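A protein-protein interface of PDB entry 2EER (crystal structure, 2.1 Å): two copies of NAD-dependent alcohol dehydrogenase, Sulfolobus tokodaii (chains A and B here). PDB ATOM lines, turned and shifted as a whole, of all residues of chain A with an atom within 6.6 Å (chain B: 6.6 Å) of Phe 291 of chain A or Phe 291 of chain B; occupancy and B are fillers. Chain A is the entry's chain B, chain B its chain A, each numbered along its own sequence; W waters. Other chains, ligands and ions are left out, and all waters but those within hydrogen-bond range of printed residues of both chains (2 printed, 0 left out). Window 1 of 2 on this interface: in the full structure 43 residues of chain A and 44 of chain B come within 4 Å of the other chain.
The backbone NH (N) of Leu 277 of chain B sits at hydrogen-bond distance from the backbone carbonyl oxygen (O) of Tyr 279 of chain A, 2.7 Å away. The backbone NH of Leu 277 of chain A is in hydrogen-bond range of the backbone carbonyl oxygen of Tyr 279 of chain B (2.8 Å). The backbone carbonyl oxygen (O) of Val 289 of chain B is in hydrogen-bond range of the backbone NH (N) of Gly 293 of chain A. The backbone NH (N) of Phe 291 of chain B is in hydrogen-bond range of the backbone carbonyl oxygen (O) of Phe 291 of chain A (2.9 Å). O of Val 289 of chain A lies within hydrogen-bond range of N of Gly 293 of chain B (3.1 Å). O of Leu 277 of chain A lies close to O of Leu 277 of chain B.
The side-chain hydroxyl (OH) of Tyr 279 of chain B is in hydrogen-bond range of the backbone carbonyl oxygen (O) of Pro 258 of chain B (3.1 Å). O of Ile 284 of chain B lies within hydrogen-bond range of N of Val 289 of chain B, at 3.2 Å. O of Pro 258 of chain A sits at hydrogen-bond distance from OH of Tyr 279 of chain A. O of Gly 265 of chain A sits at hydrogen-bond distance from N of Gln 290 of chain A, at 2.9 Å. The backbone NH (N) of Tyr 267 of chain A sits at hydrogen-bond distance from the backbone carbonyl oxygen (O) of Gln 290 of chain A (2.6 Å). O of Tyr 267 of chain A lies within hydrogen-bond range of N of Ile 292 of chain A (2.8 Å).
SD of Met 269 of chain A touches CD1 of Ile 284 of chain B, 3.8 Å away. CD2 of Leu 277 of chain A touches CD1 of Ile 284 of chain B, 3.8 Å away. Ile 284 of chain A touches Gly 293 of chain B (O to CA, 3.4 Å). O of Val 289 of chain A touches O of Phe 291 of chain B, 3.95 Å away. Gln 290 of chain A touches Phe 291 of chain B (CA to O, 3.4 Å). CG of Gln 290 of chain A touches CG2 of Ile 292 of chain B (3.9 Å). O of Phe 291 of chain A touches O of Val 289 of chain B, at 3.9 Å. Gln 290 of chain B touches Phe 291 of chain A. Gln 290 of chain B touches Ile 292 of chain A (NE2 to CG2, 3.4 Å). Gly 293 of chain A touches Ile 284 of chain B (CA to O, 3.3 Å).
Phe 291 of chain B touches three residues of chain A. Of the printed residues of chain B, Tyr 279 of chain A touches Leu 277 (2.7 Å). Of the printed residues of chain A, Ile 292 of chain B touches Val 289 (3.99 Å) and Gln 290 (3.9 Å). Of the printed residues of chain A, Val 289 of chain B touches Phe 291, Ile 292 and Gly 293. The nearest residue of chain B that does not touch Phe 291 of chain A is Ile 284 of chain B (4.7 Å). The nearest printed residue of chain A that does not touch Leu 277 of chain B is Phe 291 of chain A (5.0 Å).
Of the 17 printed residues of chain B, 9 touch a printed residue of chain A. Printed residues of chain B that touch a printed residue of chain A: Met 269, Leu 277, Tyr 279, Ile 284, Val 289, Gln 290, Phe 291, Ile 292 and Gly 293. Of the 17 printed residues of chain A, 9 touch a printed residue of chain B. Among the printed residues, no Asp or Glu carboxylate lies within 4 Å of a Lys or Arg side-chain nitrogen of the other chain.
Leu 277 of chain B touches its own counterpart, Leu 277 of chain A. Val 289 of chain A touches Phe 291 of chain B, and with the chains exchanged Phe 291 of chain A touches Val 289 of chain B. Val 289 of chain A touches Gly 293 of chain B, and with the chains exchanged Gly 293 of chain A touches Val 289 of chain B. Gln 290 of chain A touches Phe 291 of chain B, and with the chains exchanged Phe 291 of chain A touches Gln 290 of chain B.
Water W2 lies within hydrogen-bond range of O of Gly 293 of chain A and NE2 of Gln 290 of chain B. Water W1 bridges NE2 of Gln 290 of chain A (2.7 Å) and O of Gly 293 of chain B (2.9 Å).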
ATOM      1  N   LEU A 254      -8.040 -38.591 -16.982  1.00  0.00           N
ATOM      2  CA  LEU A 254      -7.627 -37.196 -16.805  1.00  0.00           C
ATOM      3  C   LEU A 254      -8.138 -36.578 -15.498  1.00  0.00           C
ATOM      4  O   LEU A 254      -7.723 -35.499 -15.092  1.00  0.00           O
ATOM      5  CB  LEU A 254      -8.166 -36.374 -17.977  1.00  0.00           C
ATOM      6  CG  LEU A 254      -7.462 -36.682 -19.299  1.00  0.00           C
ATOM      7  CD1 LEU A 254      -7.962 -35.799 -20.436  1.00  0.00           C
ATOM      8  CD2 LEU A 254      -5.946 -36.483 -19.247  1.00  0.00           C
ATOM      9  N   PRO A 258      -3.456 -36.737 -13.682  1.00  0.00           N
ATOM     10  CA  PRO A 258      -2.716 -35.472 -13.734  1.00  0.00           C
ATOM     11  C   PRO A 258      -2.414 -34.969 -12.316  1.00  0.00           C
ATOM     12  O   PRO A 258      -1.562 -34.106 -12.119  1.00  0.00           O
ATOM     13  CB  PRO A 258      -3.671 -34.550 -14.485  1.00  0.00           C
ATOM     14  CG  PRO A 258      -4.345 -35.486 -15.441  1.00  0.00           C
ATOM     15  CD  PRO A 258      -4.623 -36.708 -14.583  1.00  0.00           C
ATOM     16  N   TYR A 259      -3.116 -35.526 -11.331  1.00  0.00           N
ATOM     17  CA  TYR A 259      -2.949 -35.125  -9.932  1.00  0.00           C
ATOM     18  C   TYR A 259      -1.924 -35.921  -9.120  1.00  0.00           C
ATOM     19  O   TYR A 259      -1.740 -35.655  -7.929  1.00  0.00           O
ATOM     20  CB  TYR A 259      -4.308 -35.164  -9.226  1.00  0.00           C
ATOM     21  CG  TYR A 259      -5.301 -34.223  -9.853  1.00  0.00           C
ATOM     22  CD1 TYR A 259      -5.233 -32.849  -9.618  1.00  0.00           C
ATOM     23  CD2 TYR A 259      -6.256 -34.691 -10.753  1.00  0.00           C
ATOM     24  CE1 TYR A 259      -6.091 -31.962 -10.269  1.00  0.00           C
ATOM     25  CE2 TYR A 259      -7.114 -33.816 -11.411  1.00  0.00           C
ATOM     26  CZ  TYR A 259      -7.025 -32.452 -11.167  1.00  0.00           C
ATOM     27  OH  TYR A 259      -7.847 -31.583 -11.844  1.00  0.00           O
ATOM     28  N   LEU A 261       1.269 -36.281 -10.295  1.00  0.00           N
ATOM     29  CA  LEU A 261       2.539 -35.905 -10.906  1.00  0.00           C
ATOM     30  C   LEU A 261       3.484 -35.309  -9.878  1.00  0.00           C
ATOM     31  O   LEU A 261       3.060 -34.585  -8.981  1.00  0.00           O
ATOM     32  CB  LEU A 261       2.309 -34.864 -12.004  1.00  0.00           C
ATOM     33  CG  LEU A 261       1.706 -35.353 -13.315  1.00  0.00           C
ATOM     34  CD1 LEU A 261       1.279 -34.162 -14.156  1.00  0.00           C
ATOM     35  CD2 LEU A 261       2.741 -36.199 -14.052  1.00  0.00           C
ATOM     36  N   GLY A 265       6.923 -33.036 -13.273  1.00  0.00           N
ATOM     37  CA  GLY A 265       6.391 -34.239 -13.917  1.00  0.00           C
ATOM     38  C   GLY A 265       5.846 -33.935 -15.327  1.00  0.00           C
ATOM     39  O   GLY A 265       5.279 -32.889 -15.595  1.00  0.00           O
ATOM     40  N   LYS A 266       6.035 -34.897 -16.224  1.00  0.00           N
ATOM     41  CA  LYS A 266       5.555 -34.769 -17.591  1.00  0.00           C
ATOM     42  C   LYS A 266       4.405 -35.736 -17.867  1.00  0.00           C
ATOM     43  O   LYS A 266       4.543 -36.950 -17.708  1.00  0.00           O
ATOM     44  CB  LYS A 266       6.695 -35.040 -18.582  1.00  0.00           C
ATOM     45  CG  LYS A 266       7.861 -34.061 -18.489  1.00  0.00           C
ATOM     46  CD  LYS A 266       8.886 -34.346 -19.575  1.00  0.00           C
ATOM     47  CE  LYS A 266      10.038 -33.359 -19.538  1.00  0.00           C
ATOM     48  NZ  LYS A 266      10.762 -33.452 -18.243  1.00  0.00           N
ATOM     49  N   TYR A 267       3.267 -35.188 -18.275  1.00  0.00           N
ATOM     50  CA  TYR A 267       2.095 -35.989 -18.592  1.00  0.00           C
ATOM     51  C   TYR A 267       2.025 -36.071 -20.120  1.00  0.00           C
ATOM     52  O   TYR A 267       1.584 -35.134 -20.788  1.00  0.00           O
ATOM     53  CB  TYR A 267       0.840 -35.326 -18.011  1.00  0.00           C
ATOM     54  CG  TYR A 267      -0.325 -36.273 -17.824  1.00  0.00           C
ATOM     55  CD1 TYR A 267      -1.196 -36.569 -18.882  1.00  0.00           C
ATOM     56  CD2 TYR A 267      -0.542 -36.906 -16.598  1.00  0.00           C
ATOM     57  CE1 TYR A 267      -2.245 -37.469 -18.720  1.00  0.00           C
ATOM     58  CE2 TYR A 267      -1.584 -37.807 -16.428  1.00  0.00           C
ATOM     59  CZ  TYR A 267      -2.431 -38.086 -17.492  1.00  0.00           C
ATOM     60  OH  TYR A 267      -3.447 -38.999 -17.328  1.00  0.00           O
ATOM     61  N   VAL A 268       2.493 -37.193 -20.661  1.00  0.00           N
ATOM     62  CA  VAL A 268       2.529 -37.426 -22.105  1.00  0.00           C
ATOM     63  C   VAL A 268       1.214 -38.059 -22.535  1.00  0.00           C
ATOM     64  O   VAL A 268       0.906 -39.193 -22.173  1.00  0.00           O
ATOM     65  CB  VAL A 268       3.713 -38.350 -22.479  1.00  0.00           C
ATOM     66  CG1 VAL A 268       3.893 -38.396 -23.991  1.00  0.00           C
ATOM     67  CG2 VAL A 268       4.993 -37.840 -21.809  1.00  0.00           C
ATOM     68  N   MET A 269       0.456 -37.305 -23.321  1.00  0.00           N
ATOM     69  CA  MET A 269      -0.867 -37.699 -23.779  1.00  0.00           C
ATOM     70  C   MET A 269      -0.881 -38.339 -25.157  1.00  0.00           C
ATOM     71  O   MET A 269      -0.764 -37.662 -26.184  1.00  0.00           O
ATOM     72  CB  MET A 269      -1.766 -36.463 -23.729  1.00  0.00           C
ATOM     73  CG  MET A 269      -1.780 -35.829 -22.329  1.00  0.00           C
ATOM     74  SD  MET A 269      -2.559 -34.201 -22.223  1.00  0.00           S
ATOM     75  CE  MET A 269      -4.298 -34.677 -22.346  1.00  0.00           C
ATOM     76  N   LEU A 277      -9.224 -31.718 -21.125  1.00  0.00           N
ATOM     77  CA  LEU A 277      -8.317 -31.651 -19.991  1.00  0.00           C
ATOM     78  C   LEU A 277      -8.734 -30.395 -19.238  1.00  0.00           C
ATOM     79  O   LEU A 277      -8.746 -29.303 -19.803  1.00  0.00           O
ATOM     80  CB  LEU A 277      -6.861 -31.506 -20.459  1.00  0.00           C
ATOM     81  CG  LEU A 277      -5.825 -31.048 -19.423  1.00  0.00           C
ATOM     82  CD1 LEU A 277      -5.560 -32.166 -18.423  1.00  0.00           C
ATOM     83  CD2 LEU A 277      -4.530 -30.652 -20.124  1.00  0.00           C
ATOM     84  N   TYR A 279      -7.655 -28.490 -15.871  1.00  0.00           N
ATOM     85  CA  TYR A 279      -6.656 -28.498 -14.813  1.00  0.00           C
ATOM     86  C   TYR A 279      -6.394 -27.069 -14.337  1.00  0.00           C
ATOM     87  O   TYR A 279      -6.231 -26.163 -15.156  1.00  0.00           O
ATOM     88  CB  TYR A 279      -5.368 -29.114 -15.363  1.00  0.00           C
ATOM     89  CG  TYR A 279      -4.422 -29.654 -14.317  1.00  0.00           C
ATOM     90  CD1 TYR A 279      -4.685 -30.859 -13.669  1.00  0.00           C
ATOM     91  CD2 TYR A 279      -3.250 -28.973 -13.995  1.00  0.00           C
ATOM     92  CE1 TYR A 279      -3.796 -31.379 -12.727  1.00  0.00           C
ATOM     93  CE2 TYR A 279      -2.357 -29.479 -13.057  1.00  0.00           C
ATOM     94  CZ  TYR A 279      -2.636 -30.683 -12.428  1.00  0.00           C
ATOM     95  OH  TYR A 279      -1.752 -31.190 -11.503  1.00  0.00           O
ATOM     96  N   ILE A 284      -0.207 -25.990 -12.620  1.00  0.00           N
ATOM     97  CA  ILE A 284       0.763 -26.219 -13.681  1.00  0.00           C
ATOM     98  C   ILE A 284       2.011 -25.371 -13.447  1.00  0.00           C
ATOM     99  O   ILE A 284       3.133 -25.866 -13.485  1.00  0.00           O
ATOM    100  CB  ILE A 284       0.166 -25.865 -15.060  1.00  0.00           C
ATOM    101  CG1 ILE A 284      -1.001 -26.809 -15.374  1.00  0.00           C
ATOM    102  CG2 ILE A 284       1.248 -25.955 -16.139  1.00  0.00           C
ATOM    103  CD1 ILE A 284      -1.717 -26.511 -16.681  1.00  0.00           C
ATOM    104  N   VAL A 289       4.676 -28.583 -13.934  1.00  0.00           N
ATOM    105  CA  VAL A 289       4.184 -29.791 -14.574  1.00  0.00           C
ATOM    106  C   VAL A 289       4.068 -29.535 -16.072  1.00  0.00           C
ATOM    107  O   VAL A 289       3.994 -28.382 -16.503  1.00  0.00           O
ATOM    108  CB  VAL A 289       2.816 -30.175 -13.963  1.00  0.00           C
ATOM    109  CG1 VAL A 289       1.915 -30.831 -15.003  1.00  0.00           C
ATOM    110  CG2 VAL A 289       3.049 -31.096 -12.769  1.00  0.00           C
ATOM    111  N   GLN A 290       4.072 -30.600 -16.869  1.00  0.00           N
ATOM    112  CA  GLN A 290       3.946 -30.450 -18.312  1.00  0.00           C
ATOM    113  C   GLN A 290       2.931 -31.418 -18.911  1.00  0.00           C
ATOM    114  O   GLN A 290       2.882 -32.589 -18.541  1.00  0.00           O
ATOM    115  CB  GLN A 290       5.298 -30.676 -19.000  1.00  0.00           C
ATOM    116  CG  GLN A 290       6.370 -29.672 -18.622  1.00  0.00           C
ATOM    117  CD  GLN A 290       7.657 -29.870 -19.395  1.00  0.00           C
ATOM    118  OE1 GLN A 290       7.662 -30.457 -20.474  1.00  0.00           O
ATOM    119  NE2 GLN A 290       8.756 -29.362 -18.852  1.00  0.00           N
ATOM    120  N   PHE A 291       2.115 -30.914 -19.829  1.00  0.00           N
ATOM    121  CA  PHE A 291       1.147 -31.743 -20.536  1.00  0.00           C
ATOM    122  C   PHE A 291       1.663 -31.741 -21.966  1.00  0.00           C
ATOM    123  O   PHE A 291       1.663 -30.710 -22.639  1.00  0.00           O
ATOM    124  CB  PHE A 291      -0.254 -31.147 -20.416  1.00  0.00           C
ATOM    125  CG  PHE A 291      -0.856 -31.337 -19.052  1.00  0.00           C
ATOM    126  CD1 PHE A 291      -1.331 -32.582 -18.663  1.00  0.00           C
ATOM    127  CD2 PHE A 291      -0.885 -30.293 -18.136  1.00  0.00           C
ATOM    128  CE1 PHE A 291      -1.825 -32.793 -17.374  1.00  0.00           C
ATOM    129  CE2 PHE A 291      -1.377 -30.492 -16.844  1.00  0.00           C
ATOM    130  CZ  PHE A 291      -1.847 -31.745 -16.464  1.00  0.00           C
ATOM    131  N   ILE A 292       2.130 -32.902 -22.404  1.00  0.00           N
ATOM    132  CA  ILE A 292       2.741 -33.057 -23.718  1.00  0.00           C
ATOM    133  C   ILE A 292       2.026 -34.017 -24.658  1.00  0.00           C
ATOM    134  O   ILE A 292       1.797 -35.182 -24.319  1.00  0.00           O
ATOM    135  CB  ILE A 292       4.197 -33.559 -23.549  1.00  0.00           C
ATOM    136  CG1 ILE A 292       4.992 -32.557 -22.715  1.00  0.00           C
ATOM    137  CG2 ILE A 292       4.847 -33.786 -24.900  1.00  0.00           C
ATOM    138  CD1 ILE A 292       6.328 -33.102 -22.216  1.00  0.00           C
ATOM    139  N   GLY A 293       1.689 -33.526 -25.846  1.00  0.00           N
ATOM    140  CA  GLY A 293       1.037 -34.368 -26.826  1.00  0.00           C
ATOM    141  C   GLY A 293       2.114 -35.126 -27.583  1.00  0.00           C
ATOM    142  O   GLY A 293       3.214 -34.608 -27.800  1.00  0.00           O
ATOM    143  N   LEU B 254      -6.588 -17.786 -21.362  1.00  0.00           N
ATOM    144  CA  LEU B 254      -6.617 -19.222 -21.647  1.00  0.00           C
ATOM    145  C   LEU B 254      -7.754 -19.633 -22.595  1.00  0.00           C
ATOM    146  O   LEU B 254      -7.792 -20.744 -23.108  1.00  0.00           O
ATOM    147  CB  LEU B 254      -6.756 -19.981 -20.326  1.00  0.00           C
ATOM    148  CG  LEU B 254      -5.483 -19.923 -19.477  1.00  0.00           C
ATOM    149  CD1 LEU B 254      -5.573 -20.797 -18.231  1.00  0.00           C
ATOM    150  CD2 LEU B 254      -4.231 -20.380 -20.227  1.00  0.00           C
ATOM    151  N   PRO B 258      -4.387 -20.504 -26.352  1.00  0.00           N
ATOM    152  CA  PRO B 258      -4.055 -21.925 -26.539  1.00  0.00           C
ATOM    153  C   PRO B 258      -4.507 -22.414 -27.924  1.00  0.00           C
ATOM    154  O   PRO B 258      -3.965 -23.379 -28.466  1.00  0.00           O
ATOM    155  CB  PRO B 258      -4.830 -22.608 -25.413  1.00  0.00           C
ATOM    156  CG  PRO B 258      -4.777 -21.579 -24.322  1.00  0.00           C
ATOM    157  CD  PRO B 258      -5.046 -20.279 -25.055  1.00  0.00           C
ATOM    158  N   TYR B 259      -5.497 -21.727 -28.492  1.00  0.00           N
ATOM    159  CA  TYR B 259      -6.043 -22.088 -29.798  1.00  0.00           C
ATOM    160  C   TYR B 259      -5.288 -21.497 -30.988  1.00  0.00           C
ATOM    161  O   TYR B 259      -5.629 -21.770 -32.134  1.00  0.00           O
ATOM    162  CB  TYR B 259      -7.522 -21.684 -29.872  1.00  0.00           C
ATOM    163  CG  TYR B 259      -8.369 -22.372 -28.829  1.00  0.00           C
ATOM    164  CD1 TYR B 259      -8.772 -23.696 -28.992  1.00  0.00           C
ATOM    165  CD2 TYR B 259      -8.707 -21.723 -27.645  1.00  0.00           C
ATOM    166  CE1 TYR B 259      -9.488 -24.362 -27.995  1.00  0.00           C
ATOM    167  CE2 TYR B 259      -9.418 -22.379 -26.641  1.00  0.00           C
ATOM    168  CZ  TYR B 259      -9.803 -23.697 -26.822  1.00  0.00           C
ATOM    169  OH  TYR B 259     -10.477 -24.356 -25.818  1.00  0.00           O
ATOM    170  N   LEU B 261      -1.901 -21.851 -31.274  1.00  0.00           N
ATOM    171  CA  LEU B 261      -0.624 -22.560 -31.313  1.00  0.00           C
ATOM    172  C   LEU B 261      -0.402 -23.326 -32.614  1.00  0.00           C
ATOM    173  O   LEU B 261      -1.330 -23.929 -33.161  1.00  0.00           O
ATOM    174  CB  LEU B 261      -0.529 -23.563 -30.155  1.00  0.00           C
ATOM    175  CG  LEU B 261      -0.403 -23.079 -28.704  1.00  0.00           C
ATOM    176  CD1 LEU B 261      -0.610 -24.253 -27.761  1.00  0.00           C
ATOM    177  CD2 LEU B 261       0.969 -22.452 -28.481  1.00  0.00           C
ATOM    178  N   GLY B 265       3.619 -26.496 -30.982  1.00  0.00           N
ATOM    179  CA  GLY B 265       3.679 -25.239 -30.239  1.00  0.00           C
ATOM    180  C   GLY B 265       3.765 -25.471 -28.731  1.00  0.00           C
ATOM    181  O   GLY B 265       3.199 -26.406 -28.181  1.00  0.00           O
ATOM    182  N   LYS B 266       4.487 -24.581 -28.057  1.00  0.00           N
ATOM    183  CA  LYS B 266       4.675 -24.656 -26.612  1.00  0.00           C
ATOM    184  C   LYS B 266       4.002 -23.483 -25.901  1.00  0.00           C
ATOM    185  O   LYS B 266       4.308 -22.323 -26.176  1.00  0.00           O
ATOM    186  CB  LYS B 266       6.171 -24.659 -26.280  1.00  0.00           C
ATOM    187  CG  LYS B 266       6.935 -25.891 -26.775  1.00  0.00           C
ATOM    188  CD  LYS B 266       8.413 -25.810 -26.360  1.00  0.00           C
ATOM    189  CE  LYS B 266       9.107 -27.158 -26.444  1.00  0.00           C
ATOM    190  NZ  LYS B 266       8.998 -27.752 -27.803  1.00  0.00           N
ATOM    191  N   TYR B 267       3.082 -23.790 -24.989  1.00  0.00           N
ATOM    192  CA  TYR B 267       2.370 -22.762 -24.236  1.00  0.00           C
ATOM    193  C   TYR B 267       3.001 -22.700 -22.845  1.00  0.00           C
ATOM    194  O   TYR B 267       2.703 -23.528 -21.986  1.00  0.00           O
ATOM    195  CB  TYR B 267       0.882 -23.125 -24.123  1.00  0.00           C
ATOM    196  CG  TYR B 267      -0.020 -21.939 -23.868  1.00  0.00           C
ATOM    197  CD1 TYR B 267      -0.533 -21.187 -24.929  1.00  0.00           C
ATOM    198  CD2 TYR B 267      -0.332 -21.542 -22.566  1.00  0.00           C
ATOM    199  CE1 TYR B 267      -1.332 -20.063 -24.696  1.00  0.00           C
ATOM    200  CE2 TYR B 267      -1.132 -20.420 -22.322  1.00  0.00           C
ATOM    201  CZ  TYR B 267      -1.625 -19.686 -23.388  1.00  0.00           C
ATOM    202  OH  TYR B 267      -2.387 -18.567 -23.149  1.00  0.00           O
ATOM    203  N   VAL B 268       3.868 -21.716 -22.626  1.00  0.00           N
ATOM    204  CA  VAL B 268       4.555 -21.580 -21.347  1.00  0.00           C
ATOM    205  C   VAL B 268       3.725 -20.743 -20.393  1.00  0.00           C
ATOM    206  O   VAL B 268       3.511 -19.547 -20.614  1.00  0.00           O
ATOM    207  CB  VAL B 268       5.953 -20.942 -21.534  1.00  0.00           C
ATOM    208  CG1 VAL B 268       6.746 -21.029 -20.241  1.00  0.00           C
ATOM    209  CG2 VAL B 268       6.698 -21.656 -22.648  1.00  0.00           C
ATOM    210  N   MET B 269       3.284 -21.383 -19.316  1.00  0.00           N
ATOM    211  CA  MET B 269       2.424 -20.751 -18.328  1.00  0.00           C
ATOM    212  C   MET B 269       3.140 -20.205 -17.091  1.00  0.00           C
ATOM    213  O   MET B 269       3.524 -20.957 -16.188  1.00  0.00           O
ATOM    214  CB  MET B 269       1.341 -21.758 -17.937  1.00  0.00           C
ATOM    215  CG  MET B 269       0.602 -22.286 -19.163  1.00  0.00           C
ATOM    216  SD  MET B 269      -0.514 -23.669 -18.874  1.00  0.00           S
ATOM    217  CE  MET B 269      -1.932 -22.819 -18.209  1.00  0.00           C
ATOM    218  N   LEU B 277      -7.118 -24.436 -16.984  1.00  0.00           N
ATOM    219  CA  LEU B 277      -6.805 -24.661 -18.386  1.00  0.00           C
ATOM    220  C   LEU B 277      -7.872 -25.652 -18.834  1.00  0.00           C
ATOM    221  O   LEU B 277      -8.132 -26.634 -18.143  1.00  0.00           O
ATOM    222  CB  LEU B 277      -5.418 -25.291 -18.547  1.00  0.00           C
ATOM    223  CG  LEU B 277      -5.126 -25.878 -19.936  1.00  0.00           C
ATOM    224  CD1 LEU B 277      -5.066 -24.754 -20.971  1.00  0.00           C
ATOM    225  CD2 LEU B 277      -3.814 -26.651 -19.905  1.00  0.00           C
ATOM    226  N   TYR B 279      -8.864 -27.626 -22.387  1.00  0.00           N
ATOM    227  CA  TYR B 279      -8.503 -27.882 -23.775  1.00  0.00           C
ATOM    228  C   TYR B 279      -8.833 -29.327 -24.155  1.00  0.00           C
ATOM    229  O   TYR B 279      -8.551 -30.252 -23.390  1.00  0.00           O
ATOM    230  CB  TYR B 279      -6.998 -27.641 -23.926  1.00  0.00           C
ATOM    231  CG  TYR B 279      -6.532 -27.263 -25.308  1.00  0.00           C
ATOM    232  CD1 TYR B 279      -6.835 -26.017 -25.845  1.00  0.00           C
ATOM    233  CD2 TYR B 279      -5.760 -28.140 -26.067  1.00  0.00           C
ATOM    234  CE1 TYR B 279      -6.379 -25.648 -27.104  1.00  0.00           C
ATOM    235  CE2 TYR B 279      -5.297 -27.780 -27.329  1.00  0.00           C
ATOM    236  CZ  TYR B 279      -5.609 -26.533 -27.837  1.00  0.00           C
ATOM    237  OH  TYR B 279      -5.132 -26.156 -29.073  1.00  0.00           O
ATOM    238  N   ILE B 284      -4.423 -31.811 -28.189  1.00  0.00           N
ATOM    239  CA  ILE B 284      -3.071 -31.806 -27.634  1.00  0.00           C
ATOM    240  C   ILE B 284      -2.242 -32.907 -28.293  1.00  0.00           C
ATOM    241  O   ILE B 284      -1.093 -32.701 -28.675  1.00  0.00           O
ATOM    242  CB  ILE B 284      -3.087 -32.049 -26.103  1.00  0.00           C
ATOM    243  CG1 ILE B 284      -3.810 -30.897 -25.401  1.00  0.00           C
ATOM    244  CG2 ILE B 284      -1.651 -32.206 -25.575  1.00  0.00           C
ATOM    245  CD1 ILE B 284      -3.834 -31.011 -23.880  1.00  0.00           C
ATOM    246  N   VAL B 289       1.016 -30.345 -29.129  1.00  0.00           N
ATOM    247  CA  VAL B 289       1.286 -29.094 -28.430  1.00  0.00           C
ATOM    248  C   VAL B 289       1.654 -29.403 -26.982  1.00  0.00           C
ATOM    249  O   VAL B 289       1.439 -30.518 -26.496  1.00  0.00           O
ATOM    250  CB  VAL B 289       0.084 -28.121 -28.481  1.00  0.00           C
ATOM    251  CG1 VAL B 289      -0.078 -27.579 -29.904  1.00  0.00           C
ATOM    252  CG2 VAL B 289      -1.181 -28.816 -28.032  1.00  0.00           C
ATOM    253  N   GLN B 290       2.235 -28.430 -26.297  1.00  0.00           N
ATOM    254  CA  GLN B 290       2.627 -28.643 -24.915  1.00  0.00           C
ATOM    255  C   GLN B 290       2.235 -27.473 -24.022  1.00  0.00           C
ATOM    256  O   GLN B 290       2.381 -26.313 -24.404  1.00  0.00           O
ATOM    257  CB  GLN B 290       4.150 -28.840 -24.805  1.00  0.00           C
ATOM    258  CG  GLN B 290       4.784 -29.783 -25.821  1.00  0.00           C
ATOM    259  CD  GLN B 290       6.272 -30.018 -25.545  1.00  0.00           C
ATOM    260  OE1 GLN B 290       6.950 -29.169 -24.968  1.00  0.00           O
ATOM    261  NE2 GLN B 290       6.780 -31.168 -25.965  1.00  0.00           N
ATOM    262  N   PHE B 291       1.724 -27.787 -22.837  1.00  0.00           N
ATOM    263  CA  PHE B 291       1.380 -26.767 -21.861  1.00  0.00           C
ATOM    264  C   PHE B 291       2.442 -26.984 -20.793  1.00  0.00           C
ATOM    265  O   PHE B 291       2.475 -28.020 -20.135  1.00  0.00           O
ATOM    266  CB  PHE B 291      -0.036 -26.991 -21.342  1.00  0.00           C
ATOM    267  CG  PHE B 291      -1.089 -26.671 -22.363  1.00  0.00           C
ATOM    268  CD1 PHE B 291      -1.477 -25.354 -22.582  1.00  0.00           C
ATOM    269  CD2 PHE B 291      -1.640 -27.676 -23.150  1.00  0.00           C
ATOM    270  CE1 PHE B 291      -2.402 -25.032 -23.578  1.00  0.00           C
ATOM    271  CE2 PHE B 291      -2.564 -27.376 -24.150  1.00  0.00           C
ATOM    272  CZ  PHE B 291      -2.947 -26.048 -24.366  1.00  0.00           C
ATOM    273  N   ILE B 292       3.319 -25.995 -20.652  1.00  0.00           N
ATOM    274  CA  ILE B 292       4.464 -26.064 -19.747  1.00  0.00           C
ATOM    275  C   ILE B 292       4.486 -25.033 -18.623  1.00  0.00           C
ATOM    276  O   ILE B 292       4.449 -23.829 -18.872  1.00  0.00           O
ATOM    277  CB  ILE B 292       5.768 -25.871 -20.563  1.00  0.00           C
ATOM    278  CG1 ILE B 292       5.834 -26.901 -21.687  1.00  0.00           C
ATOM    279  CG2 ILE B 292       6.990 -25.962 -19.654  1.00  0.00           C
ATOM    280  CD1 ILE B 292       6.839 -26.541 -22.781  1.00  0.00           C
ATOM    281  N   GLY B 293       4.572 -25.507 -17.385  1.00  0.00           N
ATOM    282  CA  GLY B 293       4.634 -24.581 -16.268  1.00  0.00           C
ATOM    283  C   GLY B 293       6.076 -24.140 -16.082  1.00  0.00           C
ATOM    284  O   GLY B 293       6.994 -24.935 -16.270  1.00  0.00           O
HETATM  285  O   HOH W   1       8.122 -27.580 -16.918  1.00  0.00           O
HETATM  286  O   HOH W   2       4.805 -32.495 -28.083  1.00  0.00           O
